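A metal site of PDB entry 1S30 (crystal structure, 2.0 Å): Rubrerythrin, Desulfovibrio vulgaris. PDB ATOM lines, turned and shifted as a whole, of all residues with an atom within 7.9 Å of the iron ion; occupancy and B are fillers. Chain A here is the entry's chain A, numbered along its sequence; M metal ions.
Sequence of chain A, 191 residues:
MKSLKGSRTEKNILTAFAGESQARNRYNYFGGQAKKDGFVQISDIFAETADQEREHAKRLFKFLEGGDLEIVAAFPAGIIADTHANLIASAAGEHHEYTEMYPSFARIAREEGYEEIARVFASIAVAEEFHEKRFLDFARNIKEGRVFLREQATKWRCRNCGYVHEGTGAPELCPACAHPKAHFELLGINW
SG of Cys 161 binds the iron ion, 2.2 Å away.
The iron ion is bound by SG of Cys 174.
The iron ion is bound by the side-chain sulfur (SG) of Cys 177 (2.3 Å).
SG of Cys 158 is bound to the iron ion (2.3 Å).
The iron ion has four donor atoms within binding distance.
Four residues have an atom within 4 Å of the iron ion: Cys 158, Cys 161, Cys 174 and Cys 177.
The side-chain sulfur (SG) of Cys 158 lies close to the backbone NH (N) of Asn 160 (3.5 Å).
The side-chain sulfur (SG) of Cys 161 sits close to the backbone NH (N) of Tyr 163, 3.5 Å away.
N of Cys 158 is in hydrogen-bond range of O of Tyr 163, 2.9 Å away.
O of Cys 177 sits at hydrogen-bond distance from ND1 of His 179 (3.1 Å).
The side-chain amide oxygen (OD1) of Asn 160 sits close to the side-chain sulfur (SG) of Cys 177, 3.3 Å away.
The backbone NH (N) of Cys 174 is in hydrogen-bond range of the backbone carbonyl oxygen (O) of His 179.
The side-chain sulfur (SG) of Cys 174 lies close to the backbone NH (N) of Ala 176 (3.4 Å).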
ATOM      1  N   ARG A 157     -23.471 -31.213  33.350  1.00  0.00           N
ATOM      2  CA  ARG A 157     -24.810 -30.635  33.246  1.00  0.00           C
ATOM      3  C   ARG A 157     -24.815 -29.371  32.393  1.00  0.00           C
ATOM      4  O   ARG A 157     -23.973 -28.494  32.566  1.00  0.00           O
ATOM      5  CB  ARG A 157     -25.369 -30.306  34.647  1.00  0.00           C
ATOM      6  CG  ARG A 157     -26.839 -29.846  34.612  1.00  0.00           C
ATOM      7  CD  ARG A 157     -27.333 -29.286  35.949  1.00  0.00           C
ATOM      8  NE  ARG A 157     -26.795 -27.965  36.245  1.00  0.00           N
ATOM      9  CZ  ARG A 157     -27.538 -26.891  36.492  1.00  0.00           C
ATOM     10  NH1 ARG A 157     -28.859 -26.971  36.477  1.00  0.00           N
ATOM     11  NH2 ARG A 157     -26.951 -25.724  36.744  1.00  0.00           N
ATOM     12  N   CYS A 158     -25.767 -29.292  31.477  1.00  0.00           N
ATOM     13  CA  CYS A 158     -25.917 -28.129  30.611  1.00  0.00           C
ATOM     14  C   CYS A 158     -26.640 -27.067  31.443  1.00  0.00           C
ATOM     15  O   CYS A 158     -27.754 -27.300  31.909  1.00  0.00           O
ATOM     16  CB  CYS A 158     -26.750 -28.491  29.382  1.00  0.00           C
ATOM     17  SG  CYS A 158     -27.189 -27.060  28.357  1.00  0.00           S
ATOM     18  N   ARG A 159     -26.015 -25.911  31.602  1.00  0.00           N
ATOM     19  CA  ARG A 159     -26.616 -24.838  32.386  1.00  0.00           C
ATOM     20  C   ARG A 159     -27.854 -24.214  31.729  1.00  0.00           C
ATOM     21  O   ARG A 159     -28.708 -23.663  32.403  1.00  0.00           O
ATOM     22  CB  ARG A 159     -25.593 -23.742  32.670  1.00  0.00           C
ATOM     23  CG  ARG A 159     -24.523 -24.130  33.686  1.00  0.00           C
ATOM     24  CD  ARG A 159     -23.545 -22.976  33.912  1.00  0.00           C
ATOM     25  NE  ARG A 159     -24.200 -21.803  34.499  1.00  0.00           N
ATOM     26  CZ  ARG A 159     -24.589 -21.727  35.766  1.00  0.00           C
ATOM     27  NH1 ARG A 159     -24.404 -22.753  36.586  1.00  0.00           N
ATOM     28  NH2 ARG A 159     -25.195 -20.639  36.219  1.00  0.00           N
ATOM     29  N   ASN A 160     -27.930 -24.323  30.405  1.00  0.00           N
ATOM     30  CA  ASN A 160     -29.049 -23.753  29.674  1.00  0.00           C
ATOM     31  C   ASN A 160     -30.363 -24.531  29.783  1.00  0.00           C
ATOM     32  O   ASN A 160     -31.428 -23.922  29.940  1.00  0.00           O
ATOM     33  CB  ASN A 160     -28.663 -23.611  28.189  1.00  0.00           C
ATOM     34  CG  ASN A 160     -29.743 -22.906  27.380  1.00  0.00           C
ATOM     35  OD1 ASN A 160     -30.343 -23.501  26.481  1.00  0.00           O
ATOM     36  ND2 ASN A 160     -29.995 -21.646  27.689  1.00  0.00           N
ATOM     37  N   CYS A 161     -30.304 -25.855  29.731  1.00  0.00           N
ATOM     38  CA  CYS A 161     -31.518 -26.675  29.788  1.00  0.00           C
ATOM     39  C   CYS A 161     -31.539 -27.786  30.838  1.00  0.00           C
ATOM     40  O   CYS A 161     -32.568 -28.416  31.047  1.00  0.00           O
ATOM     41  CB  CYS A 161     -31.779 -27.312  28.417  1.00  0.00           C
ATOM     42  SG  CYS A 161     -30.686 -28.696  28.009  1.00  0.00           S
ATOM     43  N   GLY A 162     -30.407 -28.044  31.476  1.00  0.00           N
ATOM     44  CA  GLY A 162     -30.372 -29.072  32.501  1.00  0.00           C
ATOM     45  C   GLY A 162     -30.050 -30.486  32.044  1.00  0.00           C
ATOM     46  O   GLY A 162     -30.096 -31.418  32.845  1.00  0.00           O
ATOM     47  N   TYR A 163     -29.755 -30.674  30.761  1.00  0.00           N
ATOM     48  CA  TYR A 163     -29.413 -32.007  30.269  1.00  0.00           C
ATOM     49  C   TYR A 163     -28.183 -32.497  31.032  1.00  0.00           C
ATOM     50  O   TYR A 163     -27.280 -31.723  31.336  1.00  0.00           O
ATOM     51  CB  TYR A 163     -29.107 -31.964  28.774  1.00  0.00           C
ATOM     52  CG  TYR A 163     -28.647 -33.293  28.199  1.00  0.00           C
ATOM     53  CD1 TYR A 163     -29.545 -34.347  27.983  1.00  0.00           C
ATOM     54  CD2 TYR A 163     -27.297 -33.521  27.923  1.00  0.00           C
ATOM     55  CE1 TYR A 163     -29.112 -35.582  27.508  1.00  0.00           C
ATOM     56  CE2 TYR A 163     -26.859 -34.763  27.451  1.00  0.00           C
ATOM     57  CZ  TYR A 163     -27.766 -35.779  27.248  1.00  0.00           C
ATOM     58  OH  TYR A 163     -27.328 -37.000  26.797  1.00  0.00           O
ATOM     59  N   VAL A 164     -28.153 -33.786  31.354  1.00  0.00           N
ATOM     60  CA  VAL A 164     -27.015 -34.361  32.051  1.00  0.00           C
ATOM     61  C   VAL A 164     -26.288 -35.296  31.088  1.00  0.00           C
ATOM     62  O   VAL A 164     -26.902 -36.156  30.463  1.00  0.00           O
ATOM     63  CB  VAL A 164     -27.450 -35.147  33.316  1.00  0.00           C
ATOM     64  CG1 VAL A 164     -26.245 -35.859  33.931  1.00  0.00           C
ATOM     65  CG2 VAL A 164     -28.063 -34.196  34.332  1.00  0.00           C
ATOM     66  N   LEU A 173     -22.072 -30.202  21.504  1.00  0.00           N
ATOM     67  CA  LEU A 173     -23.407 -29.618  21.436  1.00  0.00           C
ATOM     68  C   LEU A 173     -24.340 -30.372  22.371  1.00  0.00           C
ATOM     69  O   LEU A 173     -24.344 -31.603  22.410  1.00  0.00           O
ATOM     70  CB  LEU A 173     -23.967 -29.714  20.015  1.00  0.00           C
ATOM     71  CG  LEU A 173     -23.322 -28.863  18.922  1.00  0.00           C
ATOM     72  CD1 LEU A 173     -23.941 -29.198  17.568  1.00  0.00           C
ATOM     73  CD2 LEU A 173     -23.507 -27.392  19.253  1.00  0.00           C
ATOM     74  N   CYS A 174     -25.137 -29.629  23.145  1.00  0.00           N
ATOM     75  CA  CYS A 174     -26.076 -30.282  24.039  1.00  0.00           C
ATOM     76  C   CYS A 174     -27.127 -30.954  23.156  1.00  0.00           C
ATOM     77  O   CYS A 174     -27.727 -30.308  22.297  1.00  0.00           O
ATOM     78  CB  CYS A 174     -26.758 -29.248  24.945  1.00  0.00           C
ATOM     79  SG  CYS A 174     -28.085 -29.966  25.959  1.00  0.00           S
ATOM     80  N   PRO A 175     -27.348 -32.261  23.347  1.00  0.00           N
ATOM     81  CA  PRO A 175     -28.340 -32.957  22.525  1.00  0.00           C
ATOM     82  C   PRO A 175     -29.795 -32.566  22.776  1.00  0.00           C
ATOM     83  O   PRO A 175     -30.676 -32.894  21.992  1.00  0.00           O
ATOM     84  CB  PRO A 175     -28.064 -34.431  22.842  1.00  0.00           C
ATOM     85  CG  PRO A 175     -27.619 -34.378  24.261  1.00  0.00           C
ATOM     86  CD  PRO A 175     -26.697 -33.189  24.286  1.00  0.00           C
ATOM     87  N   ALA A 176     -30.036 -31.859  23.879  1.00  0.00           N
ATOM     88  CA  ALA A 176     -31.391 -31.434  24.207  1.00  0.00           C
ATOM     89  C   ALA A 176     -31.735 -30.030  23.720  1.00  0.00           C
ATOM     90  O   ALA A 176     -32.773 -29.819  23.108  1.00  0.00           O
ATOM     91  CB  ALA A 176     -31.611 -31.529  25.724  1.00  0.00           C
ATOM     92  N   CYS A 177     -30.847 -29.067  23.967  1.00  0.00           N
ATOM     93  CA  CYS A 177     -31.113 -27.684  23.551  1.00  0.00           C
ATOM     94  C   CYS A 177     -30.222 -27.185  22.417  1.00  0.00           C
ATOM     95  O   CYS A 177     -30.369 -26.050  21.965  1.00  0.00           O
ATOM     96  CB  CYS A 177     -30.988 -26.744  24.755  1.00  0.00           C
ATOM     97  SG  CYS A 177     -29.300 -26.463  25.328  1.00  0.00           S
ATOM     98  N   ALA A 178     -29.315 -28.030  21.955  1.00  0.00           N
ATOM     99  CA  ALA A 178     -28.412 -27.691  20.861  1.00  0.00           C
ATOM    100  C   ALA A 178     -27.460 -26.531  21.130  1.00  0.00           C
ATOM    101  O   ALA A 178     -26.875 -25.983  20.183  1.00  0.00           O
ATOM    102  CB  ALA A 178     -29.231 -27.423  19.576  1.00  0.00           C
ATOM    103  N   HIS A 179     -27.295 -26.131  22.383  1.00  0.00           N
ATOM    104  CA  HIS A 179     -26.352 -25.055  22.670  1.00  0.00           C
ATOM    105  C   HIS A 179     -24.946 -25.632  22.719  1.00  0.00           C
ATOM    106  O   HIS A 179     -24.786 -26.826  22.953  1.00  0.00           O
ATOM    107  CB  HIS A 179     -26.698 -24.366  23.994  1.00  0.00           C
ATOM    108  CG  HIS A 179     -27.773 -23.336  23.866  1.00  0.00           C
ATOM    109  ND1 HIS A 179     -29.018 -23.631  23.331  1.00  0.00           N
ATOM    110  CD2 HIS A 179     -27.796 -22.013  24.161  1.00  0.00           C
ATOM    111  CE1 HIS A 179     -29.747 -22.530  23.302  1.00  0.00           C
ATOM    112  NE2 HIS A 179     -29.033 -21.534  23.804  1.00  0.00           N
ATOM    113  N   PRO A 180     -23.924 -24.793  22.489  1.00  0.00           N
ATOM    114  CA  PRO A 180     -22.531 -25.246  22.502  1.00  0.00           C
ATOM    115  C   PRO A 180     -21.989 -25.717  23.851  1.00  0.00           C
ATOM    116  O   PRO A 180     -22.561 -25.444  24.913  1.00  0.00           O
ATOM    117  CB  PRO A 180     -21.777 -24.051  21.950  1.00  0.00           C
ATOM    118  CG  PRO A 180     -22.586 -22.901  22.439  1.00  0.00           C
ATOM    119  CD  PRO A 180     -24.007 -23.364  22.186  1.00  0.00           C
ATOM    120  N   HIS A 183     -21.768 -24.154  27.601  1.00  0.00           N
ATOM    121  CA  HIS A 183     -22.794 -24.131  28.632  1.00  0.00           C
ATOM    122  C   HIS A 183     -22.696 -25.243  29.693  1.00  0.00           C
ATOM    123  O   HIS A 183     -23.429 -25.220  30.685  1.00  0.00           O
ATOM    124  CB  HIS A 183     -24.181 -24.170  27.967  1.00  0.00           C
ATOM    125  CG  HIS A 183     -24.508 -22.927  27.197  1.00  0.00           C
ATOM    126  ND1 HIS A 183     -25.213 -21.875  27.749  1.00  0.00           N
ATOM    127  CD2 HIS A 183     -24.188 -22.550  25.945  1.00  0.00           C
ATOM    128  CE1 HIS A 183     -25.308 -20.904  26.860  1.00  0.00           C
ATOM    129  NE2 HIS A 183     -24.696 -21.287  25.754  1.00  0.00           N
ATOM    130  N   PHE A 184     -21.804 -26.208  29.495  1.00  0.00           N
ATOM    131  CA  PHE A 184     -21.660 -27.310  30.442  1.00  0.00           C
ATOM    132  C   PHE A 184     -20.746 -27.065  31.642  1.00  0.00           C
ATOM    133  O   PHE A 184     -19.780 -26.304  31.577  1.00  0.00           O
ATOM    134  CB  PHE A 184     -21.205 -28.576  29.716  1.00  0.00           C
ATOM    135  CG  PHE A 184     -22.268 -29.202  28.867  1.00  0.00           C
ATOM    136  CD1 PHE A 184     -22.479 -28.779  27.565  1.00  0.00           C
ATOM    137  CD2 PHE A 184     -23.081 -30.205  29.393  1.00  0.00           C
ATOM    138  CE1 PHE A 184     -23.482 -29.336  26.788  1.00  0.00           C
ATOM    139  CE2 PHE A 184     -24.091 -30.774  28.625  1.00  0.00           C
ATOM    140  CZ  PHE A 184     -24.295 -30.339  27.315  1.00  0.00           C
HETATM  141 FE    FE M   1     -28.816 -28.027  26.969  1.00  0.00          FE
